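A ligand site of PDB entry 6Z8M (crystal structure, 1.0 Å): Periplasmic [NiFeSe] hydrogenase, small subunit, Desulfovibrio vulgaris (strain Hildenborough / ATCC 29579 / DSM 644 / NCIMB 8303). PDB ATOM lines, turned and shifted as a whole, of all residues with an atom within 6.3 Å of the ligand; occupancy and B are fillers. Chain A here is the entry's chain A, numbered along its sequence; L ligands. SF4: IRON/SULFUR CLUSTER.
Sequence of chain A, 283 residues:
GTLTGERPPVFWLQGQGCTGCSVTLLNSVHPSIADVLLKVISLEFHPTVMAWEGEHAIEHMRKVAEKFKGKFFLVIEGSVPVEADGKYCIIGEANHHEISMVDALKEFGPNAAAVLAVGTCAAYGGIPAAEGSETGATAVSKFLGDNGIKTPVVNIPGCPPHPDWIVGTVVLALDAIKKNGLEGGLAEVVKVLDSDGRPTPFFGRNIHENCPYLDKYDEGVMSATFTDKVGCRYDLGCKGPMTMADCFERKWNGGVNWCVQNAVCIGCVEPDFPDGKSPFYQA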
ATOM      1  N   ILE A 207     -12.242  22.781  -4.251  1.00  0.00           N
ATOM      2  CA  ILE A 207     -12.582  23.571  -5.445  1.00  0.00           C
ATOM      3  C   ILE A 207     -14.062  23.413  -5.790  1.00  0.00           C
ATOM      4  O   ILE A 207     -14.795  24.399  -5.955  1.00  0.00           O
ATOM      5  CB  ILE A 207     -11.691  23.161  -6.637  1.00  0.00           C
ATOM      6  CG1 ILE A 207     -10.206  23.449  -6.368  1.00  0.00           C
ATOM      7  CG2 ILE A 207     -12.163  23.862  -7.906  1.00  0.00           C
ATOM      8  CD1 ILE A 207      -9.738  24.870  -6.745  1.00  0.00           C
ATOM      9  N   HIS A 208     -14.501  22.172  -5.954  1.00  0.00           N
ATOM     10  CA  HIS A 208     -15.835  21.892  -6.484  1.00  0.00           C
ATOM     11  C   HIS A 208     -16.941  22.443  -5.589  1.00  0.00           C
ATOM     12  O   HIS A 208     -17.902  23.038  -6.073  1.00  0.00           O
ATOM     13  CB  HIS A 208     -15.940  20.389  -6.639  1.00  0.00           C
ATOM     14  CG  HIS A 208     -17.303  19.889  -6.990  1.00  0.00           C
ATOM     15  ND1 HIS A 208     -17.800  19.908  -8.278  1.00  0.00           N
ATOM     16  CD2 HIS A 208     -18.240  19.285  -6.225  1.00  0.00           C
ATOM     17  CE1 HIS A 208     -19.004  19.366  -8.278  1.00  0.00           C
ATOM     18  NE2 HIS A 208     -19.298  18.988  -7.047  1.00  0.00           N
ATOM     19  N   GLU A 209     -16.801  22.271  -4.273  1.00  0.00           N
ATOM     20  CA  GLU A 209     -17.859  22.728  -3.369  1.00  0.00           C
ATOM     21  C   GLU A 209     -17.984  24.243  -3.347  1.00  0.00           C
ATOM     22  O   GLU A 209     -18.993  24.752  -2.871  1.00  0.00           O
ATOM     23  CB  GLU A 209     -17.645  22.181  -1.965  1.00  0.00           C
ATOM     24  CG  GLU A 209     -17.636  20.667  -1.867  1.00  0.00           C
ATOM     25  CD  GLU A 209     -18.916  20.022  -2.393  1.00  0.00           C
ATOM     26  OE1 GLU A 209     -20.004  20.637  -2.301  1.00  0.00           O
ATOM     27  OE2 GLU A 209     -18.840  18.888  -2.898  1.00  0.00           O
ATOM     28  N   CYS A 211     -17.333  26.023  -6.349  1.00  0.00           N
ATOM     29  CA  CYS A 211     -17.182  26.376  -7.760  1.00  0.00           C
ATOM     30  C   CYS A 211     -18.404  27.135  -8.267  1.00  0.00           C
ATOM     31  O   CYS A 211     -19.541  26.767  -7.952  1.00  0.00           O
ATOM     32  CB  CYS A 211     -17.034  25.116  -8.588  1.00  0.00           C
ATOM     33  SG  CYS A 211     -16.822  25.434 -10.345  1.00  0.00           S
ATOM     34  N   PRO A 212     -18.204  28.158  -9.100  1.00  0.00           N
ATOM     35  CA  PRO A 212     -19.361  28.888  -9.653  1.00  0.00           C
ATOM     36  C   PRO A 212     -20.225  28.068 -10.576  1.00  0.00           C
ATOM     37  O   PRO A 212     -21.343  28.495 -10.864  1.00  0.00           O
ATOM     38  CB  PRO A 212     -18.707  30.082 -10.369  1.00  0.00           C
ATOM     39  CG  PRO A 212     -17.346  29.672 -10.641  1.00  0.00           C
ATOM     40  CD  PRO A 212     -16.930  28.780  -9.508  1.00  0.00           C
ATOM     41  N   TYR A 213     -19.772  26.913 -11.039  1.00  0.00           N
ATOM     42  CA  TYR A 213     -20.578  26.072 -11.915  1.00  0.00           C
ATOM     43  C   TYR A 213     -21.221  24.907 -11.174  1.00  0.00           C
ATOM     44  O   TYR A 213     -21.789  24.004 -11.796  1.00  0.00           O
ATOM     45  CB  TYR A 213     -19.738  25.594 -13.115  1.00  0.00           C
ATOM     46  CG  TYR A 213     -18.900  26.745 -13.671  1.00  0.00           C
ATOM     47  CD1 TYR A 213     -19.509  27.851 -14.250  1.00  0.00           C
ATOM     48  CD2 TYR A 213     -17.515  26.736 -13.570  1.00  0.00           C
ATOM     49  CE1 TYR A 213     -18.756  28.913 -14.725  1.00  0.00           C
ATOM     50  CE2 TYR A 213     -16.756  27.790 -14.054  1.00  0.00           C
ATOM     51  CZ  TYR A 213     -17.384  28.884 -14.626  1.00  0.00           C
ATOM     52  OH  TYR A 213     -16.641  29.933 -15.097  1.00  0.00           O
ATOM     53  N   LEU A 214     -21.183  24.934  -9.837  1.00  0.00           N
ATOM     54  CA  LEU A 214     -21.715  23.830  -9.042  1.00  0.00           C
ATOM     55  C   LEU A 214     -23.200  23.601  -9.299  1.00  0.00           C
ATOM     56  O   LEU A 214     -23.659  22.455  -9.338  1.00  0.00           O
ATOM     57  CB  LEU A 214     -21.474  24.111  -7.566  1.00  0.00           C
ATOM     58  CG  LEU A 214     -21.882  23.019  -6.584  1.00  0.00           C
ATOM     59  CD1 LEU A 214     -21.204  21.684  -6.889  1.00  0.00           C
ATOM     60  CD2 LEU A 214     -21.553  23.446  -5.162  1.00  0.00           C
ATOM     61  N   ASP A 215     -23.972  24.681  -9.476  1.00  0.00           N
ATOM     62  CA  ASP A 215     -25.382  24.492  -9.800  1.00  0.00           C
ATOM     63  C   ASP A 215     -25.558  23.709 -11.096  1.00  0.00           C
ATOM     64  O   ASP A 215     -26.439  22.842 -11.187  1.00  0.00           O
ATOM     65  CB  ASP A 215     -26.100  25.839  -9.866  1.00  0.00           C
ATOM     66  CG  ASP A 215     -26.285  26.472  -8.496  1.00  0.00           C
ATOM     67  OD1 ASP A 215     -25.971  25.829  -7.465  1.00  0.00           O
ATOM     68  OD2 ASP A 215     -26.751  27.635  -8.443  1.00  0.00           O
ATOM     69  N   LYS A 216     -24.730  23.990 -12.107  1.00  0.00           N
ATOM     70  CA  LYS A 216     -24.798  23.247 -13.355  1.00  0.00           C
ATOM     71  C   LYS A 216     -24.448  21.783 -13.153  1.00  0.00           C
ATOM     72  O   LYS A 216     -25.115  20.899 -13.701  1.00  0.00           O
ATOM     73  CB  LYS A 216     -23.892  23.876 -14.411  1.00  0.00           C
ATOM     74  CG  LYS A 216     -24.236  25.333 -14.705  1.00  0.00           C
ATOM     75  CD  LYS A 216     -25.634  25.466 -15.276  1.00  0.00           C
ATOM     76  CE  LYS A 216     -25.938  26.913 -15.577  1.00  0.00           C
ATOM     77  NZ  LYS A 216     -27.258  27.022 -16.221  1.00  0.00           N
ATOM     78  N   TYR A 217     -23.410  21.503 -12.365  1.00  0.00           N
ATOM     79  CA  TYR A 217     -23.075  20.120 -12.026  1.00  0.00           C
ATOM     80  C   TYR A 217     -24.283  19.415 -11.419  1.00  0.00           C
ATOM     81  O   TYR A 217     -24.685  18.330 -11.868  1.00  0.00           O
ATOM     82  CB  TYR A 217     -21.916  20.110 -11.031  1.00  0.00           C
ATOM     83  CG  TYR A 217     -21.572  18.732 -10.522  1.00  0.00           C
ATOM     84  CD1 TYR A 217     -20.646  17.952 -11.187  1.00  0.00           C
ATOM     85  CD2 TYR A 217     -22.146  18.232  -9.353  1.00  0.00           C
ATOM     86  CE1 TYR A 217     -20.314  16.698 -10.740  1.00  0.00           C
ATOM     87  CE2 TYR A 217     -21.812  16.972  -8.899  1.00  0.00           C
ATOM     88  CZ  TYR A 217     -20.880  16.219  -9.583  1.00  0.00           C
ATOM     89  OH  TYR A 217     -20.539  14.950  -9.138  1.00  0.00           O
ATOM     90  N   MET A 222     -23.783  19.792 -18.563  1.00  0.00           N
ATOM     91  CA  MET A 222     -22.368  19.587 -18.796  1.00  0.00           C
ATOM     92  C   MET A 222     -21.982  20.127 -20.168  1.00  0.00           C
ATOM     93  O   MET A 222     -22.630  19.792 -21.172  1.00  0.00           O
ATOM     94  CB  MET A 222     -22.045  18.098 -18.780  1.00  0.00           C
ATOM     95  CG  MET A 222     -22.351  17.441 -17.486  1.00  0.00           C
ATOM     96  SD  MET A 222     -21.240  18.056 -16.223  1.00  0.00           S
ATOM     97  CE  MET A 222     -21.945  17.205 -14.801  1.00  0.00           C
ATOM     98  N   GLY A 231     -21.921  25.471 -19.063  1.00  0.00           N
ATOM     99  CA  GLY A 231     -22.062  24.222 -18.363  1.00  0.00           C
ATOM    100  C   GLY A 231     -20.902  23.901 -17.437  1.00  0.00           C
ATOM    101  O   GLY A 231     -19.844  24.523 -17.447  1.00  0.00           O
ATOM    102  N   CYS A 232     -21.125  22.893 -16.612  1.00  0.00           N
ATOM    103  CA  CYS A 232     -20.070  22.323 -15.794  1.00  0.00           C
ATOM    104  C   CYS A 232     -19.073  21.573 -16.677  1.00  0.00           C
ATOM    105  O   CYS A 232     -19.417  21.045 -17.740  1.00  0.00           O
ATOM    106  CB  CYS A 232     -20.692  21.406 -14.740  1.00  0.00           C
ATOM    107  SG  CYS A 232     -19.597  20.268 -13.880  1.00  0.00           S
ATOM    108  N   ARG A 233     -17.814  21.568 -16.226  1.00  0.00           N
ATOM    109  CA  ARG A 233     -16.690  20.992 -16.953  1.00  0.00           C
ATOM    110  C   ARG A 233     -16.400  19.537 -16.571  1.00  0.00           C
ATOM    111  O   ARG A 233     -15.392  18.965 -17.035  1.00  0.00           O
ATOM    112  CB  ARG A 233     -15.453  21.847 -16.708  1.00  0.00           C
ATOM    113  CG  ARG A 233     -15.449  23.212 -17.400  1.00  0.00           C
ATOM    114  CD  ARG A 233     -16.453  24.234 -16.890  1.00  0.00           C
ATOM    115  NE  ARG A 233     -15.980  25.574 -17.205  1.00  0.00           N
ATOM    116  CZ  ARG A 233     -16.737  26.644 -17.425  1.00  0.00           C
ATOM    117  NH1 ARG A 233     -18.067  26.590 -17.362  1.00  0.00           N
ATOM    118  NH2 ARG A 233     -16.156  27.810 -17.696  1.00  0.00           N
ATOM    119  N   TYR A 234     -17.271  18.894 -15.791  1.00  0.00           N
ATOM    120  CA  TYR A 234     -16.980  17.561 -15.294  1.00  0.00           C
ATOM    121  C   TYR A 234     -16.752  16.551 -16.428  1.00  0.00           C
ATOM    122  O   TYR A 234     -15.831  15.730 -16.373  1.00  0.00           O
ATOM    123  CB  TYR A 234     -18.131  17.098 -14.418  1.00  0.00           C
ATOM    124  CG  TYR A 234     -17.956  15.744 -13.823  1.00  0.00           C
ATOM    125  CD1 TYR A 234     -17.141  15.542 -12.729  1.00  0.00           C
ATOM    126  CD2 TYR A 234     -18.622  14.649 -14.347  1.00  0.00           C
ATOM    127  CE1 TYR A 234     -16.993  14.300 -12.175  1.00  0.00           C
ATOM    128  CE2 TYR A 234     -18.475  13.393 -13.792  1.00  0.00           C
ATOM    129  CZ  TYR A 234     -17.650  13.225 -12.710  1.00  0.00           C
ATOM    130  OH  TYR A 234     -17.524  11.977 -12.155  1.00  0.00           O
ATOM    131  N   CYS A 238     -12.874  17.758 -15.579  1.00  0.00           N
ATOM    132  CA  CYS A 238     -12.550  18.558 -14.408  1.00  0.00           C
ATOM    133  C   CYS A 238     -12.395  17.706 -13.149  1.00  0.00           C
ATOM    134  O   CYS A 238     -13.288  16.928 -12.801  1.00  0.00           O
ATOM    135  CB  CYS A 238     -13.650  19.588 -14.187  1.00  0.00           C
ATOM    136  SG  CYS A 238     -13.260  20.771 -12.869  1.00  0.00           S
ATOM    137  N   LYS A 239     -11.277  17.897 -12.458  1.00  0.00           N
ATOM    138  CA  LYS A 239     -10.985  17.192 -11.212  1.00  0.00           C
ATOM    139  C   LYS A 239     -11.243  18.034  -9.975  1.00  0.00           C
ATOM    140  O   LYS A 239     -10.823  17.666  -8.868  1.00  0.00           O
ATOM    141  CB  LYS A 239      -9.536  16.660 -11.216  1.00  0.00           C
ATOM    142  CG  LYS A 239      -9.204  15.774 -12.418  1.00  0.00           C
ATOM    143  CD  LYS A 239     -10.228  14.646 -12.602  1.00  0.00           C
ATOM    144  CE  LYS A 239      -9.795  13.609 -13.638  1.00  0.00           C
ATOM    145  NZ  LYS A 239      -9.452  14.237 -14.914  1.00  0.00           N
ATOM    146  N   GLY A 240     -11.968  19.149 -10.118  1.00  0.00           N
ATOM    147  CA  GLY A 240     -12.361  19.943  -8.972  1.00  0.00           C
ATOM    148  C   GLY A 240     -12.918  19.165  -7.805  1.00  0.00           C
ATOM    149  O   GLY A 240     -12.620  19.497  -6.648  1.00  0.00           O
ATOM    150  N   PRO A 241     -13.754  18.144  -8.027  1.00  0.00           N
ATOM    151  CA  PRO A 241     -14.318  17.421  -6.890  1.00  0.00           C
ATOM    152  C   PRO A 241     -13.286  16.832  -5.957  1.00  0.00           C
ATOM    153  O   PRO A 241     -13.549  16.698  -4.756  1.00  0.00           O
ATOM    154  CB  PRO A 241     -15.167  16.334  -7.564  1.00  0.00           C
ATOM    155  CG  PRO A 241     -15.596  16.974  -8.847  1.00  0.00           C
ATOM    156  CD  PRO A 241     -14.388  17.754  -9.298  1.00  0.00           C
ATOM    157  N   TRP A 258      -8.716  31.416 -14.370  1.00  0.00           N
ATOM    158  CA  TRP A 258      -8.283  30.240 -13.639  1.00  0.00           C
ATOM    159  C   TRP A 258      -8.658  29.021 -14.447  1.00  0.00           C
ATOM    160  O   TRP A 258      -9.377  29.095 -15.451  1.00  0.00           O
ATOM    161  CB  TRP A 258      -8.842  30.176 -12.217  1.00  0.00           C
ATOM    162  CG  TRP A 258     -10.331  29.994 -12.090  1.00  0.00           C
ATOM    163  CD1 TRP A 258     -11.321  30.803 -12.588  1.00  0.00           C
ATOM    164  CD2 TRP A 258     -10.998  28.958 -11.361  1.00  0.00           C
ATOM    165  NE1 TRP A 258     -12.563  30.318 -12.213  1.00  0.00           N
ATOM    166  CE2 TRP A 258     -12.387  29.197 -11.441  1.00  0.00           C
ATOM    167  CE3 TRP A 258     -10.549  27.868 -10.609  1.00  0.00           C
ATOM    168  CZ2 TRP A 258     -13.324  28.375 -10.825  1.00  0.00           C
ATOM    169  CZ3 TRP A 258     -11.474  27.053  -9.990  1.00  0.00           C
ATOM    170  CH2 TRP A 258     -12.852  27.317 -10.106  1.00  0.00           C
ATOM    171  N   VAL A 260     -10.521  26.335 -14.207  1.00  0.00           N
ATOM    172  CA  VAL A 260     -11.880  25.858 -14.439  1.00  0.00           C
ATOM    173  C   VAL A 260     -12.624  26.775 -15.397  1.00  0.00           C
ATOM    174  O   VAL A 260     -13.387  26.302 -16.245  1.00  0.00           O
ATOM    175  CB  VAL A 260     -12.611  25.678 -13.106  1.00  0.00           C
ATOM    176  CG1 VAL A 260     -14.086  25.343 -13.338  1.00  0.00           C
ATOM    177  CG2 VAL A 260     -11.968  24.579 -12.290  1.00  0.00           C
ATOM    178  N   CYS A 265      -9.872  21.872 -14.272  1.00  0.00           N
ATOM    179  CA  CYS A 265      -8.888  21.620 -13.231  1.00  0.00           C
ATOM    180  C   CYS A 265      -8.326  20.228 -13.430  1.00  0.00           C
ATOM    181  O   CYS A 265      -9.055  19.269 -13.694  1.00  0.00           O
ATOM    182  CB  CYS A 265      -9.556  21.716 -11.852  1.00  0.00           C
ATOM    183  SG  CYS A 265      -8.543  21.306 -10.406  1.00  0.00           S
HETATM  184 FE1  SF4 L   1     -15.360  21.250 -12.067  1.00  0.00          FE
HETATM  185 FE2  SF4 L   1     -17.115  20.810  -9.998  1.00  0.00          FE
HETATM  186 FE3  SF4 L   1     -18.107  21.275 -12.467  1.00  0.00          FE
HETATM  187 FE4  SF4 L   1     -16.898  23.266 -11.040  1.00  0.00          FE
HETATM  188  S1  SF4 L   1     -18.862  22.238 -10.551  1.00  0.00           S
HETATM  189  S2  SF4 L   1     -16.619  22.808 -13.269  1.00  0.00           S
HETATM  190  S3  SF4 L   1     -15.235  22.095  -9.938  1.00  0.00           S
HETATM  191  S4  SF4 L   1     -16.778  19.481 -11.831  1.00  0.00           S
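SG of Cys 211 binds FE4 of the ligand, at 2.3 Å.
The backbone NH (N) of Arg 233 sits close to a sulfur (S2) of the ligand, at 3.4 Å.
FE3 of the ligand is bound by SG of Cys 232, at 2.3 Å.
A sulfur (S1) of the ligand lies close to the backbone NH (N) of Leu 214 (3.6 Å).
The side-chain sulfur (SG) of Cys 238 is bound to an iron atom (FE1) of the ligand, at 2.3 Å.
A ring nitrogen (ND1) of His 208 is bound to an iron atom (FE2) of the ligand (2.1 Å).
The backbone NH of Cys 238 lies within hydrogen-bond range of the backbone carbonyl oxygen of Arg 233 (3.1 Å).
SG of Cys 211 sits close to N of Tyr 213 (3.4 Å).
The side-chain hydroxyl (OH) of Tyr 213 lies within hydrogen-bond range of the guanidinium group (NH2) of Arg 233, at 3.4 Å.
NH1 of Arg 233 lies within hydrogen-bond range of O of Gly 231.
N of Tyr 234 lies close to SG of Cys 232 (3.3 Å).
SG of Cys 232 lies close to SD of Met 222, at 3.6 Å.
N of His 208 is in hydrogen-bond range of O of Gly 240 (3.3 Å).
NE of Arg 233 lies within hydrogen-bond range of O of Val 260 (2.9 Å).
O of Tyr 213 sits close to S1 of the ligand (3.6 Å).
Residues that only touch the ligand: Tyr 217 (3.8 Å), Tyr 234 (3.8 Å), Gly 240 (3.7 Å), Pro 241 (3.9 Å) and Val 260 (3.6 Å).
Hydrophobic or aromatic side chains within 4 Å of the ligand: His 208, Tyr 217, Tyr 234, Pro 241 and Val 260.
The nearest printed residue that does not touch the ligand is Ile 207 (4.1 Å).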
